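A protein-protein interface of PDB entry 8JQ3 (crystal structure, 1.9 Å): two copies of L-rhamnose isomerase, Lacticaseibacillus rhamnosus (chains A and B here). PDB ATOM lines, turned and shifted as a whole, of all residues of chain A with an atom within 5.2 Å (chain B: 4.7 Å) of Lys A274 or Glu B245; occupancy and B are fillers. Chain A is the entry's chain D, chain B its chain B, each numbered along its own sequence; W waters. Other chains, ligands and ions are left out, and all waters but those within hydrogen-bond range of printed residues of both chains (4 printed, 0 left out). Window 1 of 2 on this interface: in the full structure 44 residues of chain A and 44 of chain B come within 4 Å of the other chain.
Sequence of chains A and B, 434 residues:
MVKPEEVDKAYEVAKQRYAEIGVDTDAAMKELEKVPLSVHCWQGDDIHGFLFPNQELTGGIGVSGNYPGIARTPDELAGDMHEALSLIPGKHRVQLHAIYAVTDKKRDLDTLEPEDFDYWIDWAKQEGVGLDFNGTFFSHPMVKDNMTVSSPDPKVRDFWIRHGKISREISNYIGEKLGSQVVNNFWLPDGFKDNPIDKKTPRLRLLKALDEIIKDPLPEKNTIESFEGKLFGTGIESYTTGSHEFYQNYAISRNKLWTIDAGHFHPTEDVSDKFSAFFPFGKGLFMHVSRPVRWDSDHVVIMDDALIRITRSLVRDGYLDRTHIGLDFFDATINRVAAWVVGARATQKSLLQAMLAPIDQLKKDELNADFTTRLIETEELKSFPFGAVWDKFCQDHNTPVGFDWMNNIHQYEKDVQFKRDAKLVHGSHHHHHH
OE1 of Gln A248 sits at hydrogen-bond distance from ND2 of Asn B249, at 2.9 Å. NZ of Lys A274 is in salt-bridge range of OE2 of Glu B245, at 2.6 Å. The backbone carbonyl oxygen (O) of Ala A277 lies within hydrogen-bond range of the side-chain amide nitrogen (ND2) of Asn B249 (3.1 Å).
The backbone carbonyl oxygen of Glu B245 sits close to the side-chain amide nitrogen of Asn B249 (3.3 Å). The backbone NH of Phe B246 sits at hydrogen-bond distance from the side-chain hydroxyl of Ser B243 (3.0 Å). The side-chain carboxylate (OE2) of Glu A269 is in salt-bridge range of the side-chain amino group (NZ) of Lys A274 (2.7 Å).
Gln B248 touches Glu A245. NE2 of Gln A248 touches CG of Glu B245, at 3.6 Å. CE1 of His B266 touches OE2 of Glu A269, 3.4 Å away. Ala A277 touches Ser B243 (CB to OG, 3.5 Å). Glu B245 touches Ala A277. Phe B246 touches Ala A277.
Of chain B, only Glu B245 comes within 4 Å of Lys A274. Glu B245 touches just these residues of chain A: Gln A248, Lys A274 and Ala A277. Printed residues of chain B within 4 Å of Gln A248: Glu B245 and Asn B249. Of the printed residues of chain B, Ala A277 touches Ser B243 (3.5 Å), Glu B245 (3.9 Å), Phe B246 (3.7 Å) and Asn B249 (3.1 Å). Printed residues of chain B within 4 Å of Glu A269: His B266 (3.4 Å). Of the printed residues of chain A, His B266 touches Glu A269.
Along chain B the printed residues that touch a printed residue of chain A span positions 243 to 266. Printed residues of chain A that touch a printed residue of chain B: Glu A245, Gln A248, Glu A269, Lys A274 and Ala A277. Hydrophobic or aromatic side chains of chain A within 4 Å of the printed part of chain B: Ala A277. Among the printed residues, 9 pairs touch across the chains. Among the printed residues, Asp or Glu carboxylates within 4 Å of a Lys or Arg side-chain nitrogen of the other chain: Lys A274 with Glu B245.
Glu A245 touches Gln B248, and with the chains exchanged Gln A248 touches Glu B245. 2 positions are printed for both chains.
Water W1 lies within hydrogen-bond range of OE1 of Glu B245, OD2 of Asp A273 and OG of Ser B243. Water W3 lies within hydrogen-bond range of NE2 of His B266 (2.8 Å) and N of Asp A270 (2.9 Å). Water W4 lies within hydrogen-bond range of OE2 of Glu A269 and ND1 of His B266. Water W2 lies within hydrogen-bond range of NE2 of Gln A248 and NE2 of Gln B248.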
ATOM      1  N   GLU A 245      25.481 -20.277 -19.928  1.00  0.00           N
ATOM      2  CA  GLU A 245      24.178 -20.972 -19.764  1.00  0.00           C
ATOM      3  C   GLU A 245      23.175 -19.975 -19.169  1.00  0.00           C
ATOM      4  O   GLU A 245      22.058 -19.851 -19.706  1.00  0.00           O
ATOM      5  CB  GLU A 245      24.315 -22.211 -18.877  1.00  0.00           C
ATOM      6  CG  GLU A 245      24.955 -23.400 -19.575  1.00  0.00           C
ATOM      7  CD  GLU A 245      26.476 -23.354 -19.680  1.00  0.00           C
ATOM      8  OE1 GLU A 245      27.097 -22.506 -19.020  1.00  0.00           O
ATOM      9  OE2 GLU A 245      27.028 -24.174 -20.423  1.00  0.00           O
ATOM     10  N   GLN A 248      22.415 -17.248 -21.944  1.00  0.00           N
ATOM     11  CA  GLN A 248      21.585 -17.747 -23.078  1.00  0.00           C
ATOM     12  C   GLN A 248      20.134 -17.900 -22.584  1.00  0.00           C
ATOM     13  O   GLN A 248      19.217 -17.478 -23.302  1.00  0.00           O
ATOM     14  CB  GLN A 248      22.072 -19.068 -23.682  1.00  0.00           C
ATOM     15  CG  GLN A 248      21.178 -19.539 -24.828  1.00  0.00           C
ATOM     16  CD  GLN A 248      21.813 -20.497 -25.808  1.00  0.00           C
ATOM     17  OE1 GLN A 248      21.304 -20.722 -26.909  1.00  0.00           O
ATOM     18  NE2 GLN A 248      22.928 -21.085 -25.409  1.00  0.00           N
ATOM     19  N   TRP A 258      21.896 -12.274 -26.955  1.00  0.00           N
ATOM     20  CA  TRP A 258      22.941 -13.038 -26.234  1.00  0.00           C
ATOM     21  C   TRP A 258      24.288 -12.691 -26.870  1.00  0.00           C
ATOM     22  O   TRP A 258      24.360 -12.711 -28.106  1.00  0.00           O
ATOM     23  CB  TRP A 258      22.645 -14.540 -26.290  1.00  0.00           C
ATOM     24  CG  TRP A 258      23.659 -15.381 -25.582  1.00  0.00           C
ATOM     25  CD1 TRP A 258      24.309 -15.089 -24.422  1.00  0.00           C
ATOM     26  CD2 TRP A 258      24.139 -16.667 -25.999  1.00  0.00           C
ATOM     27  NE1 TRP A 258      25.173 -16.096 -24.093  1.00  0.00           N
ATOM     28  CE2 TRP A 258      25.093 -17.076 -25.045  1.00  0.00           C
ATOM     29  CE3 TRP A 258      23.870 -17.498 -27.090  1.00  0.00           C
ATOM     30  CZ2 TRP A 258      25.759 -18.293 -25.142  1.00  0.00           C
ATOM     31  CZ3 TRP A 258      24.524 -18.707 -27.180  1.00  0.00           C
ATOM     32  CH2 TRP A 258      25.461 -19.090 -26.221  1.00  0.00           C
ATOM     33  N   ILE A 260      28.138 -13.609 -27.573  1.00  0.00           N
ATOM     34  CA  ILE A 260      29.120 -14.724 -27.641  1.00  0.00           C
ATOM     35  C   ILE A 260      30.491 -14.110 -27.918  1.00  0.00           C
ATOM     36  O   ILE A 260      30.666 -13.539 -29.013  1.00  0.00           O
ATOM     37  CB  ILE A 260      28.736 -15.727 -28.737  1.00  0.00           C
ATOM     38  CG1 ILE A 260      27.352 -16.334 -28.516  1.00  0.00           C
ATOM     39  CG2 ILE A 260      29.808 -16.802 -28.874  1.00  0.00           C
ATOM     40  CD1 ILE A 260      26.867 -17.107 -29.708  1.00  0.00           C
ATOM     41  N   PHE A 265      35.362 -19.073 -23.811  1.00  0.00           N
ATOM     42  CA  PHE A 265      34.817 -20.445 -23.703  1.00  0.00           C
ATOM     43  C   PHE A 265      35.920 -21.438 -23.321  1.00  0.00           C
ATOM     44  O   PHE A 265      37.070 -21.026 -23.040  1.00  0.00           O
ATOM     45  CB  PHE A 265      34.066 -20.802 -24.985  1.00  0.00           C
ATOM     46  CG  PHE A 265      32.761 -20.058 -25.145  1.00  0.00           C
ATOM     47  CD1 PHE A 265      32.750 -18.724 -25.521  1.00  0.00           C
ATOM     48  CD2 PHE A 265      31.547 -20.686 -24.912  1.00  0.00           C
ATOM     49  CE1 PHE A 265      31.555 -18.037 -25.669  1.00  0.00           C
ATOM     50  CE2 PHE A 265      30.353 -19.996 -25.064  1.00  0.00           C
ATOM     51  CZ  PHE A 265      30.358 -18.674 -25.441  1.00  0.00           C
ATOM     52  N   GLU A 269      36.635 -25.332 -27.465  1.00  0.00           N
ATOM     53  CA  GLU A 269      35.195 -25.040 -27.668  1.00  0.00           C
ATOM     54  C   GLU A 269      35.038 -24.247 -28.965  1.00  0.00           C
ATOM     55  O   GLU A 269      35.704 -23.225 -29.110  1.00  0.00           O
ATOM     56  CB  GLU A 269      34.612 -24.288 -26.476  1.00  0.00           C
ATOM     57  CG  GLU A 269      33.100 -24.215 -26.521  1.00  0.00           C
ATOM     58  CD  GLU A 269      32.430 -24.166 -25.163  1.00  0.00           C
ATOM     59  OE1 GLU A 269      33.120 -23.919 -24.164  1.00  0.00           O
ATOM     60  OE2 GLU A 269      31.227 -24.382 -25.113  1.00  0.00           O
ATOM     61  N   ASP A 270      34.176 -24.713 -29.864  1.00  0.00           N
ATOM     62  CA  ASP A 270      33.893 -24.046 -31.156  1.00  0.00           C
ATOM     63  C   ASP A 270      32.617 -23.211 -30.998  1.00  0.00           C
ATOM     64  O   ASP A 270      31.530 -23.805 -31.063  1.00  0.00           O
ATOM     65  CB  ASP A 270      33.774 -25.084 -32.274  1.00  0.00           C
ATOM     66  CG  ASP A 270      33.453 -24.501 -33.641  1.00  0.00           C
ATOM     67  OD1 ASP A 270      33.339 -23.264 -33.739  1.00  0.00           O
ATOM     68  OD2 ASP A 270      33.307 -25.293 -34.591  1.00  0.00           O
ATOM     69  N   VAL A 271      32.747 -21.893 -30.808  1.00  0.00           N
ATOM     70  CA  VAL A 271      31.584 -20.978 -30.550  1.00  0.00           C
ATOM     71  C   VAL A 271      30.662 -20.932 -31.776  1.00  0.00           C
ATOM     72  O   VAL A 271      29.477 -20.572 -31.603  1.00  0.00           O
ATOM     73  CB  VAL A 271      32.031 -19.566 -30.116  1.00  0.00           C
ATOM     74  CG1 VAL A 271      32.821 -19.621 -28.819  1.00  0.00           C
ATOM     75  CG2 VAL A 271      32.819 -18.837 -31.198  1.00  0.00           C
ATOM     76  N   SER A 272      31.152 -21.295 -32.967  1.00  0.00           N
ATOM     77  CA  SER A 272      30.348 -21.322 -34.217  1.00  0.00           C
ATOM     78  C   SER A 272      29.263 -22.410 -34.146  1.00  0.00           C
ATOM     79  O   SER A 272      28.330 -22.359 -34.964  1.00  0.00           O
ATOM     80  CB  SER A 272      31.218 -21.475 -35.435  1.00  0.00           C
ATOM     81  OG  SER A 272      31.540 -22.832 -35.684  1.00  0.00           O
ATOM     82  N   ASP A 273      29.368 -23.351 -33.206  1.00  0.00           N
ATOM     83  CA  ASP A 273      28.363 -24.429 -32.994  1.00  0.00           C
ATOM     84  C   ASP A 273      27.090 -23.867 -32.344  1.00  0.00           C
ATOM     85  O   ASP A 273      26.054 -24.528 -32.459  1.00  0.00           O
ATOM     86  CB  ASP A 273      28.894 -25.539 -32.086  1.00  0.00           C
ATOM     87  CG  ASP A 273      27.935 -26.702 -31.872  1.00  0.00           C
ATOM     88  OD1 ASP A 273      27.585 -27.367 -32.867  1.00  0.00           O
ATOM     89  OD2 ASP A 273      27.555 -26.945 -30.701  1.00  0.00           O
ATOM     90  N   LYS A 274      27.180 -22.726 -31.658  1.00  0.00           N
ATOM     91  CA  LYS A 274      26.104 -22.226 -30.756  1.00  0.00           C
ATOM     92  C   LYS A 274      24.953 -21.594 -31.551  1.00  0.00           C
ATOM     93  O   LYS A 274      23.809 -21.670 -31.076  1.00  0.00           O
ATOM     94  CB  LYS A 274      26.653 -21.197 -29.764  1.00  0.00           C
ATOM     95  CG  LYS A 274      27.890 -21.616 -28.980  1.00  0.00           C
ATOM     96  CD  LYS A 274      27.737 -22.828 -28.087  1.00  0.00           C
ATOM     97  CE  LYS A 274      29.031 -23.144 -27.355  1.00  0.00           C
ATOM     98  NZ  LYS A 274      29.038 -24.488 -26.737  1.00  0.00           N
ATOM     99  N   PHE A 275      25.246 -20.966 -32.696  1.00  0.00           N
ATOM    100  CA  PHE A 275      24.285 -20.101 -33.431  1.00  0.00           C
ATOM    101  C   PHE A 275      23.012 -20.893 -33.741  1.00  0.00           C
ATOM    102  O   PHE A 275      21.901 -20.392 -33.454  1.00  0.00           O
ATOM    103  CB  PHE A 275      24.890 -19.532 -34.717  1.00  0.00           C
ATOM    104  CG  PHE A 275      26.288 -18.969 -34.595  1.00  0.00           C
ATOM    105  CD1 PHE A 275      26.673 -18.245 -33.479  1.00  0.00           C
ATOM    106  CD2 PHE A 275      27.197 -19.111 -35.632  1.00  0.00           C
ATOM    107  CE1 PHE A 275      27.947 -17.707 -33.383  1.00  0.00           C
ATOM    108  CE2 PHE A 275      28.465 -18.561 -35.539  1.00  0.00           C
ATOM    109  CZ  PHE A 275      28.840 -17.868 -34.414  1.00  0.00           C
ATOM    110  N   SER A 276      23.172 -22.087 -34.316  1.00  0.00           N
ATOM    111  CA  SER A 276      22.072 -22.929 -34.848  1.00  0.00           C
ATOM    112  C   SER A 276      21.333 -23.639 -33.712  1.00  0.00           C
ATOM    113  O   SER A 276      20.257 -24.190 -33.980  1.00  0.00           O
ATOM    114  CB  SER A 276      22.589 -23.913 -35.853  1.00  0.00           C
ATOM    115  OG  SER A 276      23.640 -24.692 -35.294  1.00  0.00           O
ATOM    116  N   ALA A 277      21.884 -23.631 -32.497  1.00  0.00           N
ATOM    117  CA  ALA A 277      21.204 -24.151 -31.289  1.00  0.00           C
ATOM    118  C   ALA A 277      20.436 -23.010 -30.604  1.00  0.00           C
ATOM    119  O   ALA A 277      19.559 -23.297 -29.787  1.00  0.00           O
ATOM    120  CB  ALA A 277      22.196 -24.794 -30.353  1.00  0.00           C
ATOM    121  N   PHE A 278      20.790 -21.760 -30.905  1.00  0.00           N
ATOM    122  CA  PHE A 278      20.183 -20.565 -30.269  1.00  0.00           C
ATOM    123  C   PHE A 278      18.987 -20.075 -31.092  1.00  0.00           C
ATOM    124  O   PHE A 278      17.932 -19.757 -30.504  1.00  0.00           O
ATOM    125  CB  PHE A 278      21.207 -19.442 -30.126  1.00  0.00           C
ATOM    126  CG  PHE A 278      20.614 -18.111 -29.735  1.00  0.00           C
ATOM    127  CD1 PHE A 278      20.326 -17.825 -28.410  1.00  0.00           C
ATOM    128  CD2 PHE A 278      20.350 -17.144 -30.687  1.00  0.00           C
ATOM    129  CE1 PHE A 278      19.799 -16.598 -28.041  1.00  0.00           C
ATOM    130  CE2 PHE A 278      19.818 -15.917 -30.318  1.00  0.00           C
ATOM    131  CZ  PHE A 278      19.542 -15.647 -28.996  1.00  0.00           C
ATOM    132  N   PHE A 279      19.134 -20.016 -32.415  1.00  0.00           N
ATOM    133  CA  PHE A 279      18.160 -19.317 -33.289  1.00  0.00           C
ATOM    134  C   PHE A 279      16.826 -20.061 -33.404  1.00  0.00           C
ATOM    135  O   PHE A 279      15.861 -19.444 -33.825  1.00  0.00           O
ATOM    136  CB  PHE A 279      18.778 -18.935 -34.631  1.00  0.00           C
ATOM    137  CG  PHE A 279      19.560 -17.651 -34.560  1.00  0.00           C
ATOM    138  CD1 PHE A 279      18.955 -16.482 -34.138  1.00  0.00           C
ATOM    139  CD2 PHE A 279      20.906 -17.618 -34.895  1.00  0.00           C
ATOM    140  CE1 PHE A 279      19.674 -15.300 -34.067  1.00  0.00           C
ATOM    141  CE2 PHE A 279      21.622 -16.434 -34.820  1.00  0.00           C
ATOM    142  CZ  PHE A 279      21.006 -15.278 -34.412  1.00  0.00           C
ATOM    143  N   SER B 243      22.759 -30.805 -29.431  1.00  0.00           N
ATOM    144  CA  SER B 243      23.809 -30.155 -28.609  1.00  0.00           C
ATOM    145  C   SER B 243      23.278 -29.883 -27.202  1.00  0.00           C
ATOM    146  O   SER B 243      22.043 -29.873 -27.024  1.00  0.00           O
ATOM    147  CB  SER B 243      24.300 -28.892 -29.261  1.00  0.00           C
ATOM    148  OG  SER B 243      23.309 -27.879 -29.201  1.00  0.00           O
ATOM    149  N   HIS B 244      24.173 -29.680 -26.234  1.00  0.00           N
ATOM    150  CA  HIS B 244      23.802 -29.311 -24.844  1.00  0.00           C
ATOM    151  C   HIS B 244      22.952 -28.035 -24.858  1.00  0.00           C
ATOM    152  O   HIS B 244      21.964 -27.993 -24.114  1.00  0.00           O
ATOM    153  CB  HIS B 244      25.039 -29.163 -23.957  1.00  0.00           C
ATOM    154  CG  HIS B 244      25.795 -30.435 -23.819  1.00  0.00           C
ATOM    155  ND1 HIS B 244      25.197 -31.598 -23.386  1.00  0.00           N
ATOM    156  CD2 HIS B 244      27.092 -30.729 -24.081  1.00  0.00           C
ATOM    157  CE1 HIS B 244      26.100 -32.560 -23.376  1.00  0.00           C
ATOM    158  NE2 HIS B 244      27.271 -32.053 -23.814  1.00  0.00           N
ATOM    159  N   GLU B 245      23.316 -27.047 -25.678  1.00  0.00           N
ATOM    160  CA  GLU B 245      22.578 -25.759 -25.773  1.00  0.00           C
ATOM    161  C   GLU B 245      21.190 -26.037 -26.350  1.00  0.00           C
ATOM    162  O   GLU B 245      20.179 -25.564 -25.749  1.00  0.00           O
ATOM    163  CB  GLU B 245      23.350 -24.744 -26.617  1.00  0.00           C
ATOM    164  CG  GLU B 245      24.587 -24.210 -25.922  1.00  0.00           C
ATOM    165  CD  GLU B 245      25.826 -25.082 -26.051  1.00  0.00           C
ATOM    166  OE1 GLU B 245      25.774 -26.111 -26.769  1.00  0.00           O
ATOM    167  OE2 GLU B 245      26.842 -24.728 -25.427  1.00  0.00           O
ATOM    168  N   PHE B 246      21.120 -26.786 -27.453  1.00  0.00           N
ATOM    169  CA  PHE B 246      19.829 -27.133 -28.094  1.00  0.00           C
ATOM    170  C   PHE B 246      18.885 -27.720 -27.037  1.00  0.00           C
ATOM    171  O   PHE B 246      17.741 -27.252 -26.935  1.00  0.00           O
ATOM    172  CB  PHE B 246      19.997 -28.105 -29.262  1.00  0.00           C
ATOM    173  CG  PHE B 246      18.678 -28.460 -29.898  1.00  0.00           C
ATOM    174  CD1 PHE B 246      17.899 -29.487 -29.393  1.00  0.00           C
ATOM    175  CD2 PHE B 246      18.192 -27.734 -30.969  1.00  0.00           C
ATOM    176  CE1 PHE B 246      16.677 -29.796 -29.961  1.00  0.00           C
ATOM    177  CE2 PHE B 246      16.966 -28.043 -31.536  1.00  0.00           C
ATOM    178  CZ  PHE B 246      16.206 -29.068 -31.028  1.00  0.00           C
ATOM    179  N   TYR B 247      19.337 -28.713 -26.261  1.00  0.00           N
ATOM    180  CA  TYR B 247      18.443 -29.457 -25.339  1.00  0.00           C
ATOM    181  C   TYR B 247      18.166 -28.654 -24.065  1.00  0.00           C
ATOM    182  O   TYR B 247      17.062 -28.824 -23.525  1.00  0.00           O
ATOM    183  CB  TYR B 247      18.978 -30.845 -24.990  1.00  0.00           C
ATOM    184  CG  TYR B 247      18.837 -31.870 -26.085  1.00  0.00           C
ATOM    185  CD1 TYR B 247      17.619 -32.119 -26.699  1.00  0.00           C
ATOM    186  CD2 TYR B 247      19.927 -32.619 -26.488  1.00  0.00           C
ATOM    187  CE1 TYR B 247      17.493 -33.083 -27.688  1.00  0.00           C
ATOM    188  CE2 TYR B 247      19.821 -33.583 -27.473  1.00  0.00           C
ATOM    189  CZ  TYR B 247      18.607 -33.808 -28.089  1.00  0.00           C
ATOM    190  OH  TYR B 247      18.517 -34.772 -29.047  1.00  0.00           O
ATOM    191  N   GLN B 248      19.094 -27.834 -23.566  1.00  0.00           N
ATOM    192  CA  GLN B 248      18.754 -26.983 -22.393  1.00  0.00           C
ATOM    193  C   GLN B 248      17.624 -26.039 -22.827  1.00  0.00           C
ATOM    194  O   GLN B 248      16.603 -25.916 -22.083  1.00  0.00           O
ATOM    195  CB  GLN B 248      19.958 -26.228 -21.823  1.00  0.00           C
ATOM    196  CG  GLN B 248      19.559 -25.278 -20.695  1.00  0.00           C
ATOM    197  CD  GLN B 248      20.673 -24.885 -19.759  1.00  0.00           C
ATOM    198  OE1 GLN B 248      20.430 -24.415 -18.652  1.00  0.00           O
ATOM    199  NE2 GLN B 248      21.911 -25.070 -20.194  1.00  0.00           N
ATOM    200  N   ASN B 249      17.780 -25.420 -24.001  1.00  0.00           N
ATOM    201  CA  ASN B 249      16.759 -24.523 -24.603  1.00  0.00           C
ATOM    202  C   ASN B 249      15.468 -25.315 -24.826  1.00  0.00           C
ATOM    203  O   ASN B 249      14.375 -24.784 -24.485  1.00  0.00           O
ATOM    204  CB  ASN B 249      17.252 -23.895 -25.906  1.00  0.00           C
ATOM    205  CG  ASN B 249      18.383 -22.913 -25.695  1.00  0.00           C
ATOM    206  OD1 ASN B 249      18.584 -22.414 -24.587  1.00  0.00           O
ATOM    207  ND2 ASN B 249      19.110 -22.617 -26.761  1.00  0.00           N
ATOM    208  N   HIS B 266      33.139 -30.664 -22.775  1.00  0.00           N
ATOM    209  CA  HIS B 266      34.493 -30.266 -23.241  1.00  0.00           C
ATOM    210  C   HIS B 266      35.541 -30.681 -22.223  1.00  0.00           C
ATOM    211  O   HIS B 266      35.269 -30.836 -21.037  1.00  0.00           O
ATOM    212  CB  HIS B 266      34.587 -28.760 -23.475  1.00  0.00           C
ATOM    213  CG  HIS B 266      33.803 -28.282 -24.645  1.00  0.00           C
ATOM    214  ND1 HIS B 266      32.454 -27.992 -24.552  1.00  0.00           N
ATOM    215  CD2 HIS B 266      34.169 -28.025 -25.918  1.00  0.00           C
ATOM    216  CE1 HIS B 266      32.020 -27.588 -25.727  1.00  0.00           C
ATOM    217  NE2 HIS B 266      33.058 -27.588 -26.581  1.00  0.00           N
HETATM  218  O   HOH W   1      25.313 -25.871 -29.385  1.00  0.00           O
HETATM  219  O   HOH W   2      23.063 -23.278 -22.925  1.00  0.00           O
HETATM  220  O   HOH W   3      32.277 -26.854 -29.217  1.00  0.00           O
HETATM  221  O   HOH W   4      30.157 -26.165 -23.163  1.00  0.00           O
